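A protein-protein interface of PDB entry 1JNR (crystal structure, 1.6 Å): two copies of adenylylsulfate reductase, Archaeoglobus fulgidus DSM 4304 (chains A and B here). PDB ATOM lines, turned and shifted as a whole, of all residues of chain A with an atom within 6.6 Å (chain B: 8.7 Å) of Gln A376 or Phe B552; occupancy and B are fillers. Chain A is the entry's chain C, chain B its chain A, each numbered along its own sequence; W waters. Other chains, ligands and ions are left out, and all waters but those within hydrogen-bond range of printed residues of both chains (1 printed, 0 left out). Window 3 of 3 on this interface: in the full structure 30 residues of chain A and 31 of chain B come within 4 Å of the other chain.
Water W1 bridges the backbone carbonyl oxygen (O) of Gln A376 (2.9 Å) and the guanidinium group (NH1) of Arg B545 (3.1 Å).
CZ of Phe B552 touches O of Gln A376, at 3.6 Å.
No position is printed for both chains.
Of the 6 pairs that touch across the chains among the printed residues, none has its exchanged pair printed and touching as well.
The guanidinium group (NH2) of Arg B520 lies close to the backbone carbonyl oxygen (O) of Phe B552, 3.5 Å away.
The side-chain carboxylate of Glu B548 lies within salt-bridge range of the guanidinium group of Arg B545, at 2.7 Å.
The side-chain amino group (NZ) of Lys A267 lies within salt-bridge range of the side-chain carboxylate (OD1) of Asp A268, 3.0 Å away.
The backbone NH (N) of Lys A267 lies within hydrogen-bond range of the backbone carbonyl oxygen (O) of Glu A386, at 2.8 Å.
Of chain B, only Arg B545 (3.2 Å) and Phe B552 (3.6 Å) come within 4 Å of Gln A376.
No residue of chain B comes within 4 Å of Asn A377.
Of the printed residues of chain A, Lys B523 touches Asp A268.
Ile B524 touches none of the printed residues of chain A.
Printed residues of chain A within 4 Å of Tyr B528: Lys A267 and Glu A386.
Printed residues of chain A within 4 Å of Arg B545: Gln A376 and Glu A386.
Glu B548 touches none of the printed residues of chain A.
Phe B552 touches just one residue of chain A: Gln A376 (3.6 Å).
The nearest residue of chain B that does not touch Gln A376 is Leu B549 (4.7 Å).
The nearest residue of chain A that does not touch Phe B552 is Asn A377 (4.2 Å).
The side-chain amino group (NZ) of Lys B523 is in salt-bridge range of the side-chain carboxylate (OD2) of Asp A268 (2.9 Å).
NZ of Lys A267 lies close to OH of Tyr B528, 3.4 Å away.
OE1 of Glu A386 lies within hydrogen-bond range of OH of Tyr B528 (2.5 Å).
NH2 of Arg B545 lies within hydrogen-bond range of OE1 of Gln A376 (3.2 Å).
NE of Arg B545 is in salt-bridge range of OE2 of Glu A386 (2.8 Å).
Printed residues of chain A that touch a printed residue of chain B: Lys A267, Asp A268, Gln A376 and Glu A386.
Of the 21 printed residues of chain B, 4 touch a printed residue of chain A.
Among the printed residues, 6 pairs touch across the chains.
Among the printed residues, Asp or Glu carboxylates within 4 Å of a Lys or Arg side-chain nitrogen of the other chain: Asp A268 with Lys B523 and Glu A386 with Arg B545.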
ATOM      1  N   LYS A 267     -16.972 -14.627 -12.488  1.00  0.00           N
ATOM      2  CA  LYS A 267     -17.826 -15.323 -11.529  1.00  0.00           C
ATOM      3  C   LYS A 267     -19.010 -14.515 -11.011  1.00  0.00           C
ATOM      4  O   LYS A 267     -18.906 -13.307 -10.779  1.00  0.00           O
ATOM      5  CB  LYS A 267     -16.987 -15.826 -10.340  1.00  0.00           C
ATOM      6  CG  LYS A 267     -17.752 -16.688  -9.344  1.00  0.00           C
ATOM      7  CD  LYS A 267     -16.830 -17.221  -8.250  1.00  0.00           C
ATOM      8  CE  LYS A 267     -17.608 -18.015  -7.204  1.00  0.00           C
ATOM      9  NZ  LYS A 267     -18.616 -17.166  -6.508  1.00  0.00           N
ATOM     10  N   ASP A 268     -20.136 -15.212 -10.855  1.00  0.00           N
ATOM     11  CA  ASP A 268     -21.390 -14.669 -10.331  1.00  0.00           C
ATOM     12  C   ASP A 268     -22.130 -13.646 -11.180  1.00  0.00           C
ATOM     13  O   ASP A 268     -23.334 -13.787 -11.407  1.00  0.00           O
ATOM     14  CB  ASP A 268     -21.163 -14.102  -8.927  1.00  0.00           C
ATOM     15  CG  ASP A 268     -20.914 -15.189  -7.894  1.00  0.00           C
ATOM     16  OD1 ASP A 268     -20.535 -14.850  -6.759  1.00  0.00           O
ATOM     17  OD2 ASP A 268     -21.108 -16.382  -8.213  1.00  0.00           O
ATOM     18  N   LEU A 371     -21.506  -3.696 -11.172  1.00  0.00           N
ATOM     19  CA  LEU A 371     -22.167  -3.554  -9.885  1.00  0.00           C
ATOM     20  C   LEU A 371     -21.533  -4.494  -8.864  1.00  0.00           C
ATOM     21  O   LEU A 371     -21.350  -4.131  -7.703  1.00  0.00           O
ATOM     22  CB  LEU A 371     -23.659  -3.859 -10.021  1.00  0.00           C
ATOM     23  CG  LEU A 371     -24.498  -3.675  -8.755  1.00  0.00           C
ATOM     24  CD1 LEU A 371     -24.370  -2.237  -8.262  1.00  0.00           C
ATOM     25  CD2 LEU A 371     -25.954  -4.009  -9.050  1.00  0.00           C
ATOM     26  N   LEU A 372     -21.188  -5.701  -9.301  1.00  0.00           N
ATOM     27  CA  LEU A 372     -20.567  -6.680  -8.415  1.00  0.00           C
ATOM     28  C   LEU A 372     -19.227  -6.126  -7.935  1.00  0.00           C
ATOM     29  O   LEU A 372     -18.916  -6.165  -6.744  1.00  0.00           O
ATOM     30  CB  LEU A 372     -20.372  -8.008  -9.156  1.00  0.00           C
ATOM     31  CG  LEU A 372     -19.820  -9.220  -8.394  1.00  0.00           C
ATOM     32  CD1 LEU A 372     -20.153 -10.487  -9.171  1.00  0.00           C
ATOM     33  CD2 LEU A 372     -18.311  -9.089  -8.199  1.00  0.00           C
ATOM     34  N   TRP A 373     -18.436  -5.608  -8.872  1.00  0.00           N
ATOM     35  CA  TRP A 373     -17.143  -5.024  -8.540  1.00  0.00           C
ATOM     36  C   TRP A 373     -17.324  -3.903  -7.517  1.00  0.00           C
ATOM     37  O   TRP A 373     -16.571  -3.802  -6.548  1.00  0.00           O
ATOM     38  CB  TRP A 373     -16.470  -4.467  -9.800  1.00  0.00           C
ATOM     39  CG  TRP A 373     -15.692  -5.480 -10.605  1.00  0.00           C
ATOM     40  CD1 TRP A 373     -15.485  -6.798 -10.300  1.00  0.00           C
ATOM     41  CD2 TRP A 373     -14.959  -5.229 -11.810  1.00  0.00           C
ATOM     42  NE1 TRP A 373     -14.660  -7.377 -11.238  1.00  0.00           N
ATOM     43  CE2 TRP A 373     -14.322  -6.436 -12.174  1.00  0.00           C
ATOM     44  CE3 TRP A 373     -14.774  -4.096 -12.616  1.00  0.00           C
ATOM     45  CZ2 TRP A 373     -13.514  -6.543 -13.311  1.00  0.00           C
ATOM     46  CZ3 TRP A 373     -13.970  -4.203 -13.745  1.00  0.00           C
ATOM     47  CH2 TRP A 373     -13.350  -5.418 -14.080  1.00  0.00           C
ATOM     48  N   ALA A 374     -18.335  -3.067  -7.730  1.00  0.00           N
ATOM     49  CA  ALA A 374     -18.606  -1.957  -6.824  1.00  0.00           C
ATOM     50  C   ALA A 374     -18.969  -2.450  -5.427  1.00  0.00           C
ATOM     51  O   ALA A 374     -18.460  -1.937  -4.431  1.00  0.00           O
ATOM     52  CB  ALA A 374     -19.730  -1.092  -7.380  1.00  0.00           C
ATOM     53  N   CYS A 375     -19.845  -3.447  -5.360  1.00  0.00           N
ATOM     54  CA  CYS A 375     -20.283  -4.004  -4.083  1.00  0.00           C
ATOM     55  C   CYS A 375     -19.183  -4.740  -3.325  1.00  0.00           C
ATOM     56  O   CYS A 375     -19.183  -4.764  -2.092  1.00  0.00           O
ATOM     57  CB  CYS A 375     -21.457  -4.969  -4.294  1.00  0.00           C
ATOM     58  SG  CYS A 375     -23.005  -4.199  -4.811  1.00  0.00           S
ATOM     59  N   GLN A 376     -18.256  -5.347  -4.061  1.00  0.00           N
ATOM     60  CA  GLN A 376     -17.165  -6.098  -3.454  1.00  0.00           C
ATOM     61  C   GLN A 376     -15.849  -5.321  -3.402  1.00  0.00           C
ATOM     62  O   GLN A 376     -14.799  -5.880  -3.088  1.00  0.00           O
ATOM     63  CB  GLN A 376     -16.984  -7.421  -4.206  1.00  0.00           C
ATOM     64  CG  GLN A 376     -18.134  -8.397  -3.966  1.00  0.00           C
ATOM     65  CD  GLN A 376     -18.015  -9.672  -4.777  1.00  0.00           C
ATOM     66  OE1 GLN A 376     -16.920 -10.080  -5.149  1.00  0.00           O
ATOM     67  NE2 GLN A 376     -19.148 -10.319  -5.036  1.00  0.00           N
ATOM     68  N   ASN A 377     -15.921  -4.027  -3.699  1.00  0.00           N
ATOM     69  CA  ASN A 377     -14.747  -3.159  -3.693  1.00  0.00           C
ATOM     70  C   ASN A 377     -13.590  -3.704  -4.514  1.00  0.00           C
ATOM     71  O   ASN A 377     -12.441  -3.699  -4.071  1.00  0.00           O
ATOM     72  CB  ASN A 377     -14.277  -2.903  -2.259  1.00  0.00           C
ATOM     73  CG  ASN A 377     -15.253  -2.052  -1.480  1.00  0.00           C
ATOM     74  OD1 ASN A 377     -15.873  -1.148  -2.036  1.00  0.00           O
ATOM     75  ND2 ASN A 377     -15.388  -2.326  -0.185  1.00  0.00           N
ATOM     76  N   ILE A 378     -13.895  -4.167  -5.719  1.00  0.00           N
ATOM     77  CA  ILE A 378     -12.871  -4.702  -6.599  1.00  0.00           C
ATOM     78  C   ILE A 378     -12.503  -3.685  -7.674  1.00  0.00           C
ATOM     79  O   ILE A 378     -13.337  -3.303  -8.493  1.00  0.00           O
ATOM     80  CB  ILE A 378     -13.344  -6.003  -7.287  1.00  0.00           C
ATOM     81  CG1 ILE A 378     -13.572  -7.091  -6.235  1.00  0.00           C
ATOM     82  CG2 ILE A 378     -12.314  -6.454  -8.318  1.00  0.00           C
ATOM     83  CD1 ILE A 378     -14.168  -8.372  -6.797  1.00  0.00           C
ATOM     84  N   ASP A 379     -11.254  -3.234  -7.638  1.00  0.00           N
ATOM     85  CA  ASP A 379     -10.737  -2.295  -8.622  1.00  0.00           C
ATOM     86  C   ASP A 379      -9.859  -3.147  -9.531  1.00  0.00           C
ATOM     87  O   ASP A 379      -8.806  -3.629  -9.113  1.00  0.00           O
ATOM     88  CB  ASP A 379      -9.908  -1.209  -7.938  1.00  0.00           C
ATOM     89  CG  ASP A 379      -9.324  -0.223  -8.925  1.00  0.00           C
ATOM     90  OD1 ASP A 379      -8.738   0.787  -8.480  1.00  0.00           O
ATOM     91  OD2 ASP A 379      -9.448  -0.461 -10.147  1.00  0.00           O
ATOM     92  N   GLU A 386     -12.344 -13.276  -9.898  1.00  0.00           N
ATOM     93  CA  GLU A 386     -12.573 -14.702 -10.055  1.00  0.00           C
ATOM     94  C   GLU A 386     -13.459 -14.930 -11.268  1.00  0.00           C
ATOM     95  O   GLU A 386     -14.323 -14.108 -11.588  1.00  0.00           O
ATOM     96  CB  GLU A 386     -13.252 -15.267  -8.811  1.00  0.00           C
ATOM     97  CG  GLU A 386     -12.416 -15.101  -7.558  1.00  0.00           C
ATOM     98  CD  GLU A 386     -13.184 -15.451  -6.310  1.00  0.00           C
ATOM     99  OE1 GLU A 386     -13.677 -16.593  -6.224  1.00  0.00           O
ATOM    100  OE2 GLU A 386     -13.292 -14.582  -5.421  1.00  0.00           O
ATOM    101  N   ILE B 512     -30.808  -6.167   4.602  1.00  0.00           N
ATOM    102  CA  ILE B 512     -31.009  -7.503   4.076  1.00  0.00           C
ATOM    103  C   ILE B 512     -31.942  -8.198   5.055  1.00  0.00           C
ATOM    104  O   ILE B 512     -31.883  -7.952   6.264  1.00  0.00           O
ATOM    105  CB  ILE B 512     -29.688  -8.318   3.980  1.00  0.00           C
ATOM    106  CG1 ILE B 512     -28.947  -8.292   5.319  1.00  0.00           C
ATOM    107  CG2 ILE B 512     -28.823  -7.774   2.849  1.00  0.00           C
ATOM    108  CD1 ILE B 512     -27.773  -9.256   5.383  1.00  0.00           C
ATOM    109  N   ARG B 520     -27.025 -15.950   0.957  1.00  0.00           N
ATOM    110  CA  ARG B 520     -25.652 -15.511   0.754  1.00  0.00           C
ATOM    111  C   ARG B 520     -24.671 -16.395   1.522  1.00  0.00           C
ATOM    112  O   ARG B 520     -23.645 -16.822   0.979  1.00  0.00           O
ATOM    113  CB  ARG B 520     -25.533 -14.056   1.193  1.00  0.00           C
ATOM    114  CG  ARG B 520     -24.211 -13.386   0.928  1.00  0.00           C
ATOM    115  CD  ARG B 520     -24.444 -11.888   1.023  1.00  0.00           C
ATOM    116  NE  ARG B 520     -23.251 -11.137   1.377  1.00  0.00           N
ATOM    117  CZ  ARG B 520     -23.282  -9.907   1.879  1.00  0.00           C
ATOM    118  NH1 ARG B 520     -24.447  -9.301   2.085  1.00  0.00           N
ATOM    119  NH2 ARG B 520     -22.152  -9.287   2.174  1.00  0.00           N
ATOM    120  N   LYS B 523     -24.270 -19.820  -0.142  1.00  0.00           N
ATOM    121  CA  LYS B 523     -23.520 -19.792  -1.394  1.00  0.00           C
ATOM    122  C   LYS B 523     -22.020 -19.699  -1.098  1.00  0.00           C
ATOM    123  O   LYS B 523     -21.214 -20.394  -1.712  1.00  0.00           O
ATOM    124  CB  LYS B 523     -23.977 -18.608  -2.259  1.00  0.00           C
ATOM    125  CG  LYS B 523     -23.243 -18.468  -3.593  1.00  0.00           C
ATOM    126  CD  LYS B 523     -23.839 -17.326  -4.420  1.00  0.00           C
ATOM    127  CE  LYS B 523     -22.964 -16.954  -5.619  1.00  0.00           C
ATOM    128  NZ  LYS B 523     -22.840 -18.044  -6.627  1.00  0.00           N
ATOM    129  N   ILE B 524     -21.650 -18.837  -0.157  1.00  0.00           N
ATOM    130  CA  ILE B 524     -20.251 -18.684   0.219  1.00  0.00           C
ATOM    131  C   ILE B 524     -19.677 -20.005   0.722  1.00  0.00           C
ATOM    132  O   ILE B 524     -18.620 -20.450   0.279  1.00  0.00           O
ATOM    133  CB  ILE B 524     -20.083 -17.650   1.348  1.00  0.00           C
ATOM    134  CG1 ILE B 524     -20.458 -16.259   0.839  1.00  0.00           C
ATOM    135  CG2 ILE B 524     -18.646 -17.661   1.855  1.00  0.00           C
ATOM    136  CD1 ILE B 524     -20.540 -15.222   1.939  1.00  0.00           C
ATOM    137  N   TYR B 528     -16.840 -22.155  -1.335  1.00  0.00           N
ATOM    138  CA  TYR B 528     -15.488 -22.030  -0.807  1.00  0.00           C
ATOM    139  C   TYR B 528     -15.117 -22.880   0.391  1.00  0.00           C
ATOM    140  O   TYR B 528     -13.930 -23.038   0.685  1.00  0.00           O
ATOM    141  CB  TYR B 528     -15.211 -20.574  -0.432  1.00  0.00           C
ATOM    142  CG  TYR B 528     -15.334 -19.608  -1.579  1.00  0.00           C
ATOM    143  CD1 TYR B 528     -16.545 -18.988  -1.870  1.00  0.00           C
ATOM    144  CD2 TYR B 528     -14.238 -19.331  -2.389  1.00  0.00           C
ATOM    145  CE1 TYR B 528     -16.658 -18.113  -2.945  1.00  0.00           C
ATOM    146  CE2 TYR B 528     -14.340 -18.464  -3.466  1.00  0.00           C
ATOM    147  CZ  TYR B 528     -15.550 -17.859  -3.739  1.00  0.00           C
ATOM    148  OH  TYR B 528     -15.643 -17.013  -4.819  1.00  0.00           O
ATOM    149  N   ARG B 545     -10.695 -16.828   0.804  1.00  0.00           N
ATOM    150  CA  ARG B 545     -11.686 -16.008   0.122  1.00  0.00           C
ATOM    151  C   ARG B 545     -12.991 -16.099   0.903  1.00  0.00           C
ATOM    152  O   ARG B 545     -13.732 -15.122   1.003  1.00  0.00           O
ATOM    153  CB  ARG B 545     -11.886 -16.480  -1.322  1.00  0.00           C
ATOM    154  CG  ARG B 545     -12.895 -15.654  -2.118  1.00  0.00           C
ATOM    155  CD  ARG B 545     -12.631 -14.157  -2.006  1.00  0.00           C
ATOM    156  NE  ARG B 545     -13.450 -13.388  -2.942  1.00  0.00           N
ATOM    157  CZ  ARG B 545     -13.650 -12.076  -2.860  1.00  0.00           C
ATOM    158  NH1 ARG B 545     -13.096 -11.376  -1.881  1.00  0.00           N
ATOM    159  NH2 ARG B 545     -14.398 -11.460  -3.764  1.00  0.00           N
ATOM    160  N   ALA B 546     -13.265 -17.271   1.466  1.00  0.00           N
ATOM    161  CA  ALA B 546     -14.475 -17.454   2.257  1.00  0.00           C
ATOM    162  C   ALA B 546     -14.472 -16.471   3.422  1.00  0.00           C
ATOM    163  O   ALA B 546     -15.488 -15.849   3.721  1.00  0.00           O
ATOM    164  CB  ALA B 546     -14.559 -18.885   2.783  1.00  0.00           C
ATOM    165  N   LEU B 547     -13.326 -16.328   4.081  1.00  0.00           N
ATOM    166  CA  LEU B 547     -13.240 -15.410   5.212  1.00  0.00           C
ATOM    167  C   LEU B 547     -13.501 -13.978   4.760  1.00  0.00           C
ATOM    168  O   LEU B 547     -14.140 -13.203   5.471  1.00  0.00           O
ATOM    169  CB  LEU B 547     -11.872 -15.530   5.895  1.00  0.00           C
ATOM    170  CG  LEU B 547     -11.640 -16.882   6.584  1.00  0.00           C
ATOM    171  CD1 LEU B 547     -10.252 -16.921   7.202  1.00  0.00           C
ATOM    172  CD2 LEU B 547     -12.706 -17.105   7.644  1.00  0.00           C
ATOM    173  N   GLU B 548     -13.019 -13.635   3.570  1.00  0.00           N
ATOM    174  CA  GLU B 548     -13.235 -12.301   3.026  1.00  0.00           C
ATOM    175  C   GLU B 548     -14.717 -12.067   2.769  1.00  0.00           C
ATOM    176  O   GLU B 548     -15.261 -11.013   3.107  1.00  0.00           O
ATOM    177  CB  GLU B 548     -12.460 -12.128   1.720  1.00  0.00           C
ATOM    178  CG  GLU B 548     -10.967 -11.924   1.902  1.00  0.00           C
ATOM    179  CD  GLU B 548     -10.216 -11.938   0.584  1.00  0.00           C
ATOM    180  OE1 GLU B 548     -10.824 -11.598  -0.454  1.00  0.00           O
ATOM    181  OE2 GLU B 548      -9.015 -12.277   0.587  1.00  0.00           O
ATOM    182  N   LEU B 549     -15.382 -13.052   2.177  1.00  0.00           N
ATOM    183  CA  LEU B 549     -16.801 -12.900   1.890  1.00  0.00           C
ATOM    184  C   LEU B 549     -17.642 -12.938   3.162  1.00  0.00           C
ATOM    185  O   LEU B 549     -18.659 -12.259   3.252  1.00  0.00           O
ATOM    186  CB  LEU B 549     -17.260 -13.972   0.899  1.00  0.00           C
ATOM    187  CG  LEU B 549     -16.588 -13.858  -0.478  1.00  0.00           C
ATOM    188  CD1 LEU B 549     -17.054 -15.008  -1.373  1.00  0.00           C
ATOM    189  CD2 LEU B 549     -16.918 -12.510  -1.113  1.00  0.00           C
ATOM    190  N   LEU B 550     -17.216 -13.725   4.146  1.00  0.00           N
ATOM    191  CA  LEU B 550     -17.941 -13.801   5.410  1.00  0.00           C
ATOM    192  C   LEU B 550     -17.785 -12.483   6.164  1.00  0.00           C
ATOM    193  O   LEU B 550     -18.649 -12.103   6.949  1.00  0.00           O
ATOM    194  CB  LEU B 550     -17.414 -14.954   6.266  1.00  0.00           C
ATOM    195  CG  LEU B 550     -17.827 -16.363   5.832  1.00  0.00           C
ATOM    196  CD1 LEU B 550     -17.057 -17.394   6.648  1.00  0.00           C
ATOM    197  CD2 LEU B 550     -19.332 -16.541   6.014  1.00  0.00           C
ATOM    198  N   ALA B 551     -16.676 -11.789   5.919  1.00  0.00           N
ATOM    199  CA  ALA B 551     -16.422 -10.507   6.568  1.00  0.00           C
ATOM    200  C   ALA B 551     -17.438  -9.490   6.060  1.00  0.00           C
ATOM    201  O   ALA B 551     -17.996  -8.719   6.841  1.00  0.00           O
ATOM    202  CB  ALA B 551     -15.003 -10.035   6.271  1.00  0.00           C
ATOM    203  N   PHE B 552     -17.677  -9.490   4.751  1.00  0.00           N
ATOM    204  CA  PHE B 552     -18.656  -8.579   4.160  1.00  0.00           C
ATOM    205  C   PHE B 552     -20.032  -8.908   4.737  1.00  0.00           C
ATOM    206  O   PHE B 552     -20.795  -8.016   5.107  1.00  0.00           O
ATOM    207  CB  PHE B 552     -18.729  -8.758   2.638  1.00  0.00           C
ATOM    208  CG  PHE B 552     -17.616  -8.092   1.871  1.00  0.00           C
ATOM    209  CD1 PHE B 552     -16.962  -8.780   0.852  1.00  0.00           C
ATOM    210  CD2 PHE B 552     -17.281  -6.760   2.100  1.00  0.00           C
ATOM    211  CE1 PHE B 552     -15.997  -8.153   0.067  1.00  0.00           C
ATOM    212  CE2 PHE B 552     -16.314  -6.122   1.318  1.00  0.00           C
ATOM    213  CZ  PHE B 552     -15.673  -6.822   0.299  1.00  0.00           C
ATOM    214  N   LEU B 553     -20.349 -10.199   4.795  1.00  0.00           N
ATOM    215  CA  LEU B 553     -21.638 -10.630   5.314  1.00  0.00           C
ATOM    216  C   LEU B 553     -21.803 -10.239   6.773  1.00  0.00           C
ATOM    217  O   LEU B 553     -22.857  -9.745   7.176  1.00  0.00           O
ATOM    218  CB  LEU B 553     -21.799 -12.148   5.161  1.00  0.00           C
ATOM    219  CG  LEU B 553     -23.123 -12.725   5.675  1.00  0.00           C
ATOM    220  CD1 LEU B 553     -24.303 -12.016   5.015  1.00  0.00           C
ATOM    221  CD2 LEU B 553     -23.175 -14.215   5.391  1.00  0.00           C
ATOM    222  N   LYS B 554     -20.755 -10.447   7.560  1.00  0.00           N
ATOM    223  CA  LYS B 554     -20.803 -10.108   8.975  1.00  0.00           C
ATOM    224  C   LYS B 554     -21.089  -8.615   9.138  1.00  0.00           C
ATOM    225  O   LYS B 554     -21.888  -8.213   9.981  1.00  0.00           O
ATOM    226  CB  LYS B 554     -19.477 -10.473   9.646  1.00  0.00           C
ATOM    227  CG  LYS B 554     -19.470 -10.223  11.149  1.00  0.00           C
ATOM    228  CD  LYS B 554     -18.092 -10.440  11.755  1.00  0.00           C
ATOM    229  CE  LYS B 554     -17.585 -11.852  11.535  1.00  0.00           C
ATOM    230  NZ  LYS B 554     -16.236 -12.010  12.138  1.00  0.00           N
ATOM    231  N   GLU B 555     -20.441  -7.790   8.324  1.00  0.00           N
ATOM    232  CA  GLU B 555     -20.667  -6.350   8.395  1.00  0.00           C
ATOM    233  C   GLU B 555     -22.116  -6.038   8.030  1.00  0.00           C
ATOM    234  O   GLU B 555     -22.750  -5.169   8.636  1.00  0.00           O
ATOM    235  CB  GLU B 555     -19.724  -5.608   7.443  1.00  0.00           C
ATOM    236  CG  GLU B 555     -18.252  -5.848   7.730  1.00  0.00           C
ATOM    237  CD  GLU B 555     -17.337  -5.104   6.777  1.00  0.00           C
ATOM    238  OE1 GLU B 555     -17.619  -5.099   5.559  1.00  0.00           O
ATOM    239  OE2 GLU B 555     -16.327  -4.533   7.241  1.00  0.00           O
ATOM    240  N   ASP B 556     -22.646  -6.756   7.043  1.00  0.00           N
ATOM    241  CA  ASP B 556     -24.020  -6.535   6.610  1.00  0.00           C
ATOM    242  C   ASP B 556     -25.060  -7.021   7.615  1.00  0.00           C
ATOM    243  O   ASP B 556     -26.233  -6.656   7.522  1.00  0.00           O
ATOM    244  CB  ASP B 556     -24.260  -7.185   5.243  1.00  0.00           C
ATOM    245  CG  ASP B 556     -23.560  -6.445   4.117  1.00  0.00           C
ATOM    246  OD1 ASP B 556     -23.018  -5.342   4.360  1.00  0.00           O
ATOM    247  OD2 ASP B 556     -23.555  -6.963   2.979  1.00  0.00           O
ATOM    248  N   LEU B 557     -24.641  -7.842   8.573  1.00  0.00           N
ATOM    249  CA  LEU B 557     -25.568  -8.315   9.593  1.00  0.00           C
ATOM    250  C   LEU B 557     -25.990  -7.111  10.430  1.00  0.00           C
ATOM    251  O   LEU B 557     -27.058  -7.114  11.046  1.00  0.00           O
ATOM    252  CB  LEU B 557     -24.910  -9.363  10.492  1.00  0.00           C
ATOM    253  CG  LEU B 557     -24.608 -10.718   9.851  1.00  0.00           C
ATOM    254  CD1 LEU B 557     -23.931 -11.616  10.868  1.00  0.00           C
ATOM    255  CD2 LEU B 557     -25.898 -11.353   9.354  1.00  0.00           C
ATOM    256  N   GLU B 558     -25.141  -6.086  10.451  1.00  0.00           N
ATOM    257  CA  GLU B 558     -25.444  -4.869  11.197  1.00  0.00           C
ATOM    258  C   GLU B 558     -26.570  -4.119  10.500  1.00  0.00           C
ATOM    259  O   GLU B 558     -27.116  -3.153  11.034  1.00  0.00           O
ATOM    260  CB  GLU B 558     -24.206  -3.973  11.297  1.00  0.00           C
ATOM    261  CG  GLU B 558     -23.053  -4.596  12.075  1.00  0.00           C
ATOM    262  CD  GLU B 558     -23.459  -5.027  13.474  1.00  0.00           C
ATOM    263  OE1 GLU B 558     -23.926  -4.169  14.254  1.00  0.00           O
ATOM    264  OE2 GLU B 558     -23.312  -6.225  13.799  1.00  0.00           O
ATOM    265  N   LYS B 559     -26.912  -4.567   9.296  1.00  0.00           N
ATOM    266  CA  LYS B 559     -27.987  -3.951   8.539  1.00  0.00           C
ATOM    267  C   LYS B 559     -29.113  -4.949   8.272  1.00  0.00           C
ATOM    268  O   LYS B 559     -29.789  -4.891   7.249  1.00  0.00           O
ATOM    269  CB  LYS B 559     -27.442  -3.360   7.232  1.00  0.00           C
ATOM    270  CG  LYS B 559     -26.531  -2.161   7.461  1.00  0.00           C
ATOM    271  CD  LYS B 559     -26.363  -1.303   6.218  1.00  0.00           C
ATOM    272  CE  LYS B 559     -25.470  -0.097   6.517  1.00  0.00           C
ATOM    273  NZ  LYS B 559     -25.373   0.862   5.375  1.00  0.00           N
ATOM    274  N   VAL B 578     -23.712 -17.515  10.859  1.00  0.00           N
ATOM    275  CA  VAL B 578     -22.571 -16.846  10.245  1.00  0.00           C
ATOM    276  C   VAL B 578     -21.301 -17.016  11.072  1.00  0.00           C
ATOM    277  O   VAL B 578     -20.241 -17.338  10.530  1.00  0.00           O
ATOM    278  CB  VAL B 578     -22.847 -15.341  10.022  1.00  0.00           C
ATOM    279  CG1 VAL B 578     -21.585 -14.646   9.527  1.00  0.00           C
ATOM    280  CG2 VAL B 578     -23.959 -15.169   9.000  1.00  0.00           C
HETATM  281  O   HOH W   1     -13.966  -8.589  -2.787  1.00  0.00           O
